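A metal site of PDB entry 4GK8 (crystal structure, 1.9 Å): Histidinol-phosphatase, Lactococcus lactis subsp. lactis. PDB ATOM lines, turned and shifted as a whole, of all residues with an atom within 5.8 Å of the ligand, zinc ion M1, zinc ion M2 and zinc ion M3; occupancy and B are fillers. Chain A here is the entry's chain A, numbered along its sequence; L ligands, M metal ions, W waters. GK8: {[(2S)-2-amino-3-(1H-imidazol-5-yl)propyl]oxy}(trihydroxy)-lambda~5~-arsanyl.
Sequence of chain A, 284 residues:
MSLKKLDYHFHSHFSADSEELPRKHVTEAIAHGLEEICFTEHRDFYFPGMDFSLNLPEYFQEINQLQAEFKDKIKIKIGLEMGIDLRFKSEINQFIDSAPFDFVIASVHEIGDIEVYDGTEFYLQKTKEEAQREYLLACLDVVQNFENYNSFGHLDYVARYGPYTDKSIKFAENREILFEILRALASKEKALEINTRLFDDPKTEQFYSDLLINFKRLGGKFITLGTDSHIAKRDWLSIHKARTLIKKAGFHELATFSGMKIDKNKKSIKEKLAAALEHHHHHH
An oxygen (O1) of the ligand is in hydrogen-bond range of the guanidinium group of Arg 160, at 2.4 Å.
The side-chain carboxylate (OE2) of Glu 115 lies within hydrogen-bond range of a nitrogen (ND1) of the ligand, 2.6 Å away.
The guanidinium group (NH2) of Arg 197 sits at hydrogen-bond distance from an oxygen (O1) of the ligand.
A nitrogen (N) of the ligand is in hydrogen-bond range of the side-chain hydroxyl (OH) of Tyr 157 (3.3 Å).
A ring nitrogen (ND1) of His 109 lies within hydrogen-bond range of the side-chain carboxylate (OD2) of Asp 44.
O of His 109 is in hydrogen-bond range of N of Val 116, at 3.0 Å.
N of His 42 sits at hydrogen-bond distance from OG of Ser 15 (2.9 Å).
A ring nitrogen (ND1) of His 11 sits close to the backbone carbonyl oxygen (O) of Thr 40 (3.3 Å).
A ring nitrogen (ND1) of His 11 lies within hydrogen-bond range of the side-chain hydroxyl (OG) of Ser 15, 3.1 Å away.
The side-chain carboxylate of Asp 228 is in salt-bridge range of the guanidinium group of Arg 197 (3.9 Å).
The side-chain carboxylate (OD2) of Asp 228 lies within hydrogen-bond range of the side-chain amide nitrogen (ND2) of Asn 195.
O of Phe 52 lies within hydrogen-bond range of N of Asp 44 (3.2 Å).
Residues that only touch the ligand: Tyr 117 (3.8 Å), Phe 52 (3.9 Å) and Met 50 (3.96 Å).
Hydrophobic or aromatic side chains that line the ligand: His 11, His 42, Met 50, Phe 52, His 109, Tyr 117, Tyr 157 and His 230.
Of the 25 residues printed, 16 come within 4 Å of the ligand.
Within 4 Å of zinc ion M1: Asp 17, His 42 and His 230.
Along chain A the residues within 4 Å of zinc ion M1 span positions 17 to 230.
The nearest printed residue that does not touch zinc ion M1 is His 11 (4.1 Å).
OG of Ser 107 touches zinc ion M2 (3.9 Å).
Tyr 157 touches zinc ion M2 (CE1 to ZN, 3.99 Å).
Five residues have an atom within 4 Å of zinc ion M2: Glu 81, Ser 107, His 109, His 154 and Tyr 157.
NE2 of His 42 binds zinc ion M1 (2.1 Å).
Zinc ion M1 is bound by OD2 of Asp 17 (2.1 Å).
A ring nitrogen (NE2) of His 230 is bound to zinc ion M1 (2.1 Å).
O4 of the ligand is bound to zinc ion M1, 2.2 Å away.
Slightly farther from zinc ion M1 lies O3 of the ligand (2.7 Å).
Zinc ion M2 is bound by O2 of the ligand, OE2 of Glu 81, water W1, NE2 of His 109 and NE2 of His 154.
O3 of the ligand binds zinc ion M3, at 1.8 Å.
Water W1 binds zinc ion M3 (2.1 Å).
NE2 of His 9 binds zinc ion M3 (2.1 Å).
A ring nitrogen (NE2) of His 11 is bound to zinc ion M3, at 2.2 Å.
OE1 of Glu 81 is bound to zinc ion M3 (2.2 Å).
Zinc ion M3 is bound by OD1 of Asp 228 (2.3 Å).
Water W1 lies within hydrogen-bond range of OD2 of Asp 228 (2.6 Å) and O1 of the ligand (3.2 Å).
Water W2 lies within hydrogen-bond range of a nitrogen (N) of the ligand (2.6 Å), the side-chain carboxylate (OD1) of Asp 44 (3.0 Å) and a ring nitrogen (ND1) of His 109 (3.4 Å).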
ATOM      1  N   HIS A   9       1.724  16.171  18.749  1.00  0.00           N
ATOM      2  CA  HIS A   9       3.158  16.455  18.723  1.00  0.00           C
ATOM      3  C   HIS A   9       3.491  17.467  19.816  1.00  0.00           C
ATOM      4  O   HIS A   9       3.173  18.640  19.687  1.00  0.00           O
ATOM      5  CB  HIS A   9       3.588  17.004  17.350  1.00  0.00           C
ATOM      6  CG  HIS A   9       5.073  17.114  17.165  1.00  0.00           C
ATOM      7  ND1 HIS A   9       5.668  17.098  15.925  1.00  0.00           N
ATOM      8  CD2 HIS A   9       6.088  17.219  18.067  1.00  0.00           C
ATOM      9  CE1 HIS A   9       6.982  17.212  16.071  1.00  0.00           C
ATOM     10  NE2 HIS A   9       7.260  17.279  17.359  1.00  0.00           N
ATOM     11  N   PHE A  10       4.122  16.996  20.888  1.00  0.00           N
ATOM     12  CA  PHE A  10       4.566  17.902  21.956  1.00  0.00           C
ATOM     13  C   PHE A  10       5.534  17.191  22.888  1.00  0.00           C
ATOM     14  O   PHE A  10       5.657  15.955  22.866  1.00  0.00           O
ATOM     15  CB  PHE A  10       3.372  18.538  22.716  1.00  0.00           C
ATOM     16  CG  PHE A  10       2.468  17.539  23.395  1.00  0.00           C
ATOM     17  CD1 PHE A  10       2.688  17.171  24.720  1.00  0.00           C
ATOM     18  CD2 PHE A  10       1.381  17.001  22.723  1.00  0.00           C
ATOM     19  CE1 PHE A  10       1.860  16.258  25.352  1.00  0.00           C
ATOM     20  CE2 PHE A  10       0.554  16.092  23.342  1.00  0.00           C
ATOM     21  CZ  PHE A  10       0.792  15.715  24.665  1.00  0.00           C
ATOM     22  N   HIS A  11       6.243  17.977  23.699  1.00  0.00           N
ATOM     23  CA  HIS A  11       7.393  17.488  24.451  1.00  0.00           C
ATOM     24  C   HIS A  11       7.350  17.904  25.911  1.00  0.00           C
ATOM     25  O   HIS A  11       6.902  19.014  26.228  1.00  0.00           O
ATOM     26  CB  HIS A  11       8.664  18.058  23.833  1.00  0.00           C
ATOM     27  CG  HIS A  11       8.841  17.698  22.389  1.00  0.00           C
ATOM     28  ND1 HIS A  11       9.558  16.596  21.985  1.00  0.00           N
ATOM     29  CD2 HIS A  11       8.391  18.285  21.259  1.00  0.00           C
ATOM     30  CE1 HIS A  11       9.556  16.519  20.672  1.00  0.00           C
ATOM     31  NE2 HIS A  11       8.848  17.531  20.201  1.00  0.00           N
ATOM     32  N   SER A  15      12.067  14.836  27.137  1.00  0.00           N
ATOM     33  CA  SER A  15      12.846  15.238  25.963  1.00  0.00           C
ATOM     34  C   SER A  15      14.016  16.103  26.378  1.00  0.00           C
ATOM     35  O   SER A  15      13.897  16.890  27.319  1.00  0.00           O
ATOM     36  CB  SER A  15      11.982  16.046  24.984  1.00  0.00           C
ATOM     37  OG  SER A  15      11.012  15.232  24.342  1.00  0.00           O
ATOM     38  N   ASP A  17      15.301  18.740  25.158  1.00  0.00           N
ATOM     39  CA  ASP A  17      15.191  20.184  24.980  1.00  0.00           C
ATOM     40  C   ASP A  17      13.891  20.760  25.560  1.00  0.00           C
ATOM     41  O   ASP A  17      13.444  21.826  25.145  1.00  0.00           O
ATOM     42  CB  ASP A  17      15.321  20.573  23.505  1.00  0.00           C
ATOM     43  CG  ASP A  17      14.194  20.036  22.644  1.00  0.00           C
ATOM     44  OD1 ASP A  17      13.440  19.180  23.129  1.00  0.00           O
ATOM     45  OD2 ASP A  17      14.070  20.454  21.448  1.00  0.00           O
ATOM     46  N   THR A  40       5.056  13.037  22.376  1.00  0.00           N
ATOM     47  CA  THR A  40       5.963  12.570  21.334  1.00  0.00           C
ATOM     48  C   THR A  40       7.386  13.011  21.651  1.00  0.00           C
ATOM     49  O   THR A  40       7.923  13.912  21.012  1.00  0.00           O
ATOM     50  CB  THR A  40       5.571  13.081  19.915  1.00  0.00           C
ATOM     51  OG1 THR A  40       5.556  14.504  19.895  1.00  0.00           O
ATOM     52  CG2 THR A  40       4.185  12.560  19.484  1.00  0.00           C
ATOM     53  N   HIS A  42      11.511  13.272  22.211  1.00  0.00           N
ATOM     54  CA  HIS A  42      12.659  13.107  21.298  1.00  0.00           C
ATOM     55  C   HIS A  42      13.498  11.867  21.541  1.00  0.00           C
ATOM     56  O   HIS A  42      13.935  11.617  22.685  1.00  0.00           O
ATOM     57  CB  HIS A  42      13.634  14.284  21.478  1.00  0.00           C
ATOM     58  CG  HIS A  42      13.193  15.570  20.838  1.00  0.00           C
ATOM     59  ND1 HIS A  42      12.943  15.676  19.482  1.00  0.00           N
ATOM     60  CD2 HIS A  42      13.023  16.805  21.356  1.00  0.00           C
ATOM     61  CE1 HIS A  42      12.616  16.921  19.204  1.00  0.00           C
ATOM     62  NE2 HIS A  42      12.661  17.625  20.319  1.00  0.00           N
ATOM     63  N   ASP A  44      17.001  11.021  19.139  1.00  0.00           N
ATOM     64  CA  ASP A  44      17.858  11.210  17.961  1.00  0.00           C
ATOM     65  C   ASP A  44      19.203  10.542  18.289  1.00  0.00           C
ATOM     66  O   ASP A  44      19.795  10.857  19.314  1.00  0.00           O
ATOM     67  CB  ASP A  44      18.133  12.706  17.700  1.00  0.00           C
ATOM     68  CG  ASP A  44      16.866  13.505  17.340  1.00  0.00           C
ATOM     69  OD1 ASP A  44      16.081  13.836  18.265  1.00  0.00           O
ATOM     70  OD2 ASP A  44      16.678  13.846  16.151  1.00  0.00           O
ATOM     71  N   PHE A  47      23.389  12.546  18.038  1.00  0.00           N
ATOM     72  CA  PHE A  47      23.049  13.884  17.581  1.00  0.00           C
ATOM     73  C   PHE A  47      24.218  14.826  17.774  1.00  0.00           C
ATOM     74  O   PHE A  47      24.902  14.743  18.786  1.00  0.00           O
ATOM     75  CB  PHE A  47      21.821  14.442  18.304  1.00  0.00           C
ATOM     76  CG  PHE A  47      21.131  15.557  17.561  1.00  0.00           C
ATOM     77  CD1 PHE A  47      20.372  15.265  16.432  1.00  0.00           C
ATOM     78  CD2 PHE A  47      21.279  16.876  17.948  1.00  0.00           C
ATOM     79  CE1 PHE A  47      19.733  16.276  15.727  1.00  0.00           C
ATOM     80  CE2 PHE A  47      20.647  17.899  17.248  1.00  0.00           C
ATOM     81  CZ  PHE A  47      19.874  17.599  16.137  1.00  0.00           C
ATOM     82  N   MET A  50      24.551  17.764  21.195  1.00  0.00           N
ATOM     83  CA  MET A  50      23.625  17.608  22.304  1.00  0.00           C
ATOM     84  C   MET A  50      22.949  16.245  22.253  1.00  0.00           C
ATOM     85  O   MET A  50      22.478  15.819  21.201  1.00  0.00           O
ATOM     86  CB  MET A  50      22.565  18.706  22.219  1.00  0.00           C
ATOM     87  CG  MET A  50      21.460  18.609  23.258  1.00  0.00           C
ATOM     88  SD  MET A  50      20.313  19.977  23.002  1.00  0.00           S
ATOM     89  CE  MET A  50      19.090  19.604  24.244  1.00  0.00           C
ATOM     90  N   PHE A  52      20.154  13.595  22.573  1.00  0.00           N
ATOM     91  CA  PHE A  52      18.706  13.445  22.651  1.00  0.00           C
ATOM     92  C   PHE A  52      18.357  12.008  23.000  1.00  0.00           C
ATOM     93  O   PHE A  52      17.950  11.219  22.154  1.00  0.00           O
ATOM     94  CB  PHE A  52      18.030  13.874  21.329  1.00  0.00           C
ATOM     95  CG  PHE A  52      17.878  15.360  21.192  1.00  0.00           C
ATOM     96  CD1 PHE A  52      16.719  15.993  21.616  1.00  0.00           C
ATOM     97  CD2 PHE A  52      18.897  16.125  20.661  1.00  0.00           C
ATOM     98  CE1 PHE A  52      16.572  17.359  21.492  1.00  0.00           C
ATOM     99  CE2 PHE A  52      18.745  17.504  20.533  1.00  0.00           C
ATOM    100  CZ  PHE A  52      17.589  18.120  20.953  1.00  0.00           C
ATOM    101  N   GLU A  81       8.933  11.167  18.850  1.00  0.00           N
ATOM    102  CA  GLU A  81       9.445  11.859  17.674  1.00  0.00           C
ATOM    103  C   GLU A  81      10.842  11.347  17.408  1.00  0.00           C
ATOM    104  O   GLU A  81      11.783  11.664  18.135  1.00  0.00           O
ATOM    105  CB  GLU A  81       9.445  13.389  17.820  1.00  0.00           C
ATOM    106  CG  GLU A  81       9.898  14.058  16.504  1.00  0.00           C
ATOM    107  CD  GLU A  81      10.129  15.561  16.601  1.00  0.00           C
ATOM    108  OE1 GLU A  81      10.040  16.144  17.694  1.00  0.00           O
ATOM    109  OE2 GLU A  81      10.410  16.164  15.533  1.00  0.00           O
ATOM    110  N   SER A 107      11.232  12.428  11.609  1.00  0.00           N
ATOM    111  CA  SER A 107      11.640  13.807  11.388  1.00  0.00           C
ATOM    112  C   SER A 107      13.084  13.843  10.920  1.00  0.00           C
ATOM    113  O   SER A 107      13.879  12.972  11.274  1.00  0.00           O
ATOM    114  CB  SER A 107      11.564  14.590  12.698  1.00  0.00           C
ATOM    115  OG  SER A 107      10.219  14.815  13.098  1.00  0.00           O
ATOM    116  N   HIS A 109      16.307  16.192  11.442  1.00  0.00           N
ATOM    117  CA  HIS A 109      16.835  17.247  12.312  1.00  0.00           C
ATOM    118  C   HIS A 109      18.305  17.553  12.042  1.00  0.00           C
ATOM    119  O   HIS A 109      18.833  18.604  12.432  1.00  0.00           O
ATOM    120  CB  HIS A 109      16.690  16.850  13.783  1.00  0.00           C
ATOM    121  CG  HIS A 109      15.273  16.779  14.256  1.00  0.00           C
ATOM    122  ND1 HIS A 109      14.821  15.787  15.097  1.00  0.00           N
ATOM    123  CD2 HIS A 109      14.203  17.584  14.013  1.00  0.00           C
ATOM    124  CE1 HIS A 109      13.534  15.977  15.347  1.00  0.00           C
ATOM    125  NE2 HIS A 109      13.133  17.059  14.709  1.00  0.00           N
ATOM    126  N   GLU A 115      23.661  19.859  12.264  1.00  0.00           N
ATOM    127  CA  GLU A 115      22.299  20.129  12.706  1.00  0.00           C
ATOM    128  C   GLU A 115      21.619  21.233  11.887  1.00  0.00           C
ATOM    129  O   GLU A 115      22.220  22.262  11.580  1.00  0.00           O
ATOM    130  CB  GLU A 115      22.272  20.506  14.199  1.00  0.00           C
ATOM    131  CG  GLU A 115      20.870  20.822  14.691  1.00  0.00           C
ATOM    132  CD  GLU A 115      20.827  21.237  16.151  1.00  0.00           C
ATOM    133  OE1 GLU A 115      21.883  21.540  16.726  1.00  0.00           O
ATOM    134  OE2 GLU A 115      19.715  21.252  16.710  1.00  0.00           O
ATOM    135  N   VAL A 116      20.369  20.999  11.512  1.00  0.00           N
ATOM    136  CA  VAL A 116      19.561  22.025  10.864  1.00  0.00           C
ATOM    137  C   VAL A 116      18.963  22.889  11.977  1.00  0.00           C
ATOM    138  O   VAL A 116      17.994  22.498  12.622  1.00  0.00           O
ATOM    139  CB  VAL A 116      18.448  21.389   9.993  1.00  0.00           C
ATOM    140  CG1 VAL A 116      17.631  22.475   9.268  1.00  0.00           C
ATOM    141  CG2 VAL A 116      19.063  20.409   9.001  1.00  0.00           C
ATOM    142  N   TYR A 117      19.551  24.055  12.224  1.00  0.00           N
ATOM    143  CA  TYR A 117      19.154  24.863  13.365  1.00  0.00           C
ATOM    144  C   TYR A 117      19.802  26.221  13.270  1.00  0.00           C
ATOM    145  O   TYR A 117      20.693  26.411  12.461  1.00  0.00           O
ATOM    146  CB  TYR A 117      19.561  24.187  14.678  1.00  0.00           C
ATOM    147  CG  TYR A 117      18.726  24.636  15.862  1.00  0.00           C
ATOM    148  CD1 TYR A 117      17.407  24.209  16.001  1.00  0.00           C
ATOM    149  CD2 TYR A 117      19.258  25.465  16.845  1.00  0.00           C
ATOM    150  CE1 TYR A 117      16.627  24.608  17.076  1.00  0.00           C
ATOM    151  CE2 TYR A 117      18.480  25.868  17.929  1.00  0.00           C
ATOM    152  CZ  TYR A 117      17.170  25.442  18.031  1.00  0.00           C
ATOM    153  OH  TYR A 117      16.392  25.825  19.101  1.00  0.00           O
ATOM    154  N   HIS A 154       6.960  17.858  10.426  1.00  0.00           N
ATOM    155  CA  HIS A 154       7.318  19.204   9.965  1.00  0.00           C
ATOM    156  C   HIS A 154       8.156  19.332   8.682  1.00  0.00           C
ATOM    157  O   HIS A 154       9.361  19.535   8.736  1.00  0.00           O
ATOM    158  CB  HIS A 154       7.980  20.014  11.117  1.00  0.00           C
ATOM    159  CG  HIS A 154       9.095  19.296  11.827  1.00  0.00           C
ATOM    160  ND1 HIS A 154      10.122  18.648  11.169  1.00  0.00           N
ATOM    161  CD2 HIS A 154       9.349  19.143  13.145  1.00  0.00           C
ATOM    162  CE1 HIS A 154      10.964  18.136  12.059  1.00  0.00           C
ATOM    163  NE2 HIS A 154      10.521  18.421  13.268  1.00  0.00           N
ATOM    164  N   TYR A 157      10.324  22.424   8.499  1.00  0.00           N
ATOM    165  CA  TYR A 157      11.307  22.591   9.577  1.00  0.00           C
ATOM    166  C   TYR A 157      12.449  23.539   9.193  1.00  0.00           C
ATOM    167  O   TYR A 157      12.874  24.390   9.986  1.00  0.00           O
ATOM    168  CB  TYR A 157      11.863  21.219   9.982  1.00  0.00           C
ATOM    169  CG  TYR A 157      12.771  21.178  11.200  1.00  0.00           C
ATOM    170  CD1 TYR A 157      12.245  21.187  12.489  1.00  0.00           C
ATOM    171  CD2 TYR A 157      14.155  21.048  11.052  1.00  0.00           C
ATOM    172  CE1 TYR A 157      13.079  21.110  13.598  1.00  0.00           C
ATOM    173  CE2 TYR A 157      14.992  20.979  12.158  1.00  0.00           C
ATOM    174  CZ  TYR A 157      14.442  21.011  13.422  1.00  0.00           C
ATOM    175  OH  TYR A 157      15.268  20.943  14.519  1.00  0.00           O
ATOM    176  N   ARG A 160      12.170  27.286   9.764  1.00  0.00           N
ATOM    177  CA  ARG A 160      12.171  27.871  11.097  1.00  0.00           C
ATOM    178  C   ARG A 160      13.446  28.660  11.353  1.00  0.00           C
ATOM    179  O   ARG A 160      13.453  29.577  12.169  1.00  0.00           O
ATOM    180  CB  ARG A 160      12.040  26.803  12.172  1.00  0.00           C
ATOM    181  CG  ARG A 160      10.760  25.971  12.104  1.00  0.00           C
ATOM    182  CD  ARG A 160      10.892  24.813  13.090  1.00  0.00           C
ATOM    183  NE  ARG A 160       9.658  24.037  13.208  1.00  0.00           N
ATOM    184  CZ  ARG A 160       9.474  23.125  14.159  1.00  0.00           C
ATOM    185  NH1 ARG A 160      10.446  22.919  15.043  1.00  0.00           N
ATOM    186  NH2 ARG A 160       8.327  22.454  14.231  1.00  0.00           N
ATOM    187  N   TYR A 161      14.530  28.290  10.688  1.00  0.00           N
ATOM    188  CA  TYR A 161      15.856  28.717  11.141  1.00  0.00           C
ATOM    189  C   TYR A 161      16.676  29.295  10.007  1.00  0.00           C
ATOM    190  O   TYR A 161      16.286  29.232   8.852  1.00  0.00           O
ATOM    191  CB  TYR A 161      16.621  27.547  11.782  1.00  0.00           C
ATOM    192  CG  TYR A 161      15.785  26.694  12.717  1.00  0.00           C
ATOM    193  CD1 TYR A 161      15.397  27.182  13.962  1.00  0.00           C
ATOM    194  CD2 TYR A 161      15.383  25.408  12.349  1.00  0.00           C
ATOM    195  CE1 TYR A 161      14.616  26.401  14.829  1.00  0.00           C
ATOM    196  CE2 TYR A 161      14.603  24.632  13.204  1.00  0.00           C
ATOM    197  CZ  TYR A 161      14.232  25.131  14.438  1.00  0.00           C
ATOM    198  OH  TYR A 161      13.456  24.363  15.288  1.00  0.00           O
ATOM    199  N   ASN A 195       2.077  20.743  11.197  1.00  0.00           N
ATOM    200  CA  ASN A 195       2.792  21.221  12.377  1.00  0.00           C
ATOM    201  C   ASN A 195       2.533  22.712  12.539  1.00  0.00           C
ATOM    202  O   ASN A 195       2.820  23.488  11.634  1.00  0.00           O
ATOM    203  CB  ASN A 195       4.297  20.939  12.197  1.00  0.00           C
ATOM    204  CG  ASN A 195       5.093  21.191  13.466  1.00  0.00           C
ATOM    205  OD1 ASN A 195       5.055  22.280  14.036  1.00  0.00           O
ATOM    206  ND2 ASN A 195       5.821  20.178  13.909  1.00  0.00           N
ATOM    207  N   ARG A 197       3.817  25.059  14.506  1.00  0.00           N
ATOM    208  CA  ARG A 197       4.859  25.911  15.077  1.00  0.00           C
ATOM    209  C   ARG A 197       4.907  27.321  14.461  1.00  0.00           C
ATOM    210  O   ARG A 197       4.876  28.310  15.193  1.00  0.00           O
ATOM    211  CB  ARG A 197       6.239  25.251  14.999  1.00  0.00           C
ATOM    212  CG  ARG A 197       7.389  26.207  15.405  1.00  0.00           C
ATOM    213  CD  ARG A 197       7.416  26.535  16.901  1.00  0.00           C
ATOM    214  NE  ARG A 197       7.644  25.332  17.708  1.00  0.00           N
ATOM    215  CZ  ARG A 197       8.830  24.739  17.853  1.00  0.00           C
ATOM    216  NH1 ARG A 197       9.903  25.232  17.258  1.00  0.00           N
ATOM    217  NH2 ARG A 197       8.930  23.630  18.583  1.00  0.00           N
ATOM    218  N   ASP A 228       3.851  21.003  18.405  1.00  0.00           N
ATOM    219  CA  ASP A 228       5.285  20.977  18.693  1.00  0.00           C
ATOM    220  C   ASP A 228       5.645  21.802  19.943  1.00  0.00           C
ATOM    221  O   ASP A 228       6.751  22.321  20.057  1.00  0.00           O
ATOM    222  CB  ASP A 228       6.113  21.455  17.497  1.00  0.00           C
ATOM    223  CG  ASP A 228       7.392  20.646  17.308  1.00  0.00           C
ATOM    224  OD1 ASP A 228       7.853  19.982  18.263  1.00  0.00           O
ATOM    225  OD2 ASP A 228       7.931  20.675  16.190  1.00  0.00           O
ATOM    226  N   HIS A 230       6.875  22.811  23.531  1.00  0.00           N
ATOM    227  CA  HIS A 230       7.822  22.309  24.508  1.00  0.00           C
ATOM    228  C   HIS A 230       7.458  22.840  25.896  1.00  0.00           C
ATOM    229  O   HIS A 230       8.092  22.495  26.883  1.00  0.00           O
ATOM    230  CB  HIS A 230       9.251  22.687  24.131  1.00  0.00           C
ATOM    231  CG  HIS A 230       9.749  21.952  22.919  1.00  0.00           C
ATOM    232  ND1 HIS A 230       9.077  21.963  21.719  1.00  0.00           N
ATOM    233  CD2 HIS A 230      10.846  21.184  22.735  1.00  0.00           C
ATOM    234  CE1 HIS A 230       9.745  21.233  20.845  1.00  0.00           C
ATOM    235  NE2 HIS A 230      10.827  20.751  21.436  1.00  0.00           N
HETATM  236  C   GK8 L   1      14.121  20.946  18.018  1.00  0.00           C
HETATM  237  N   GK8 L   1      15.136  18.956  17.097  1.00  0.00           N
HETATM  238 AS   GK8 L   1      11.551  20.058  17.594  1.00  0.00          AS
HETATM  239  O1  GK8 L   1      10.889  21.598  17.042  1.00  0.00           O
HETATM  240  O2  GK8 L   1      12.338  19.087  16.321  1.00  0.00           O
HETATM  241  O3  GK8 L   1      10.531  19.074  18.650  1.00  0.00           O
HETATM  242  O4  GK8 L   1      12.937  20.563  18.625  1.00  0.00           O
HETATM  243  CA  GK8 L   1      15.294  20.000  18.074  1.00  0.00           C
HETATM  244  CB  GK8 L   1      16.594  20.711  17.827  1.00  0.00           C
HETATM  245  CG  GK8 L   1      17.273  21.406  18.964  1.00  0.00           C
HETATM  246  ND1 GK8 L   1      18.586  21.744  19.042  1.00  0.00           N
HETATM  247  CD2 GK8 L   1      16.690  21.836  20.157  1.00  0.00           C
HETATM  248  CE1 GK8 L   1      18.812  22.351  20.208  1.00  0.00           C
HETATM  249  NE2 GK8 L   1      17.665  22.409  20.883  1.00  0.00           N
HETATM  250 ZN    ZN M   1      12.375  19.678  20.509  1.00  0.00          ZN
HETATM  251 ZN    ZN M   2      11.299  17.910  15.185  1.00  0.00          ZN
HETATM  252 ZN    ZN M   3       9.071  18.090  18.126  1.00  0.00          ZN
HETATM  253  O   HOH W   1       9.702  18.705  16.217  1.00  0.00           O
HETATM  254  O   HOH W   2      16.140  16.791  18.077  1.00  0.00           O
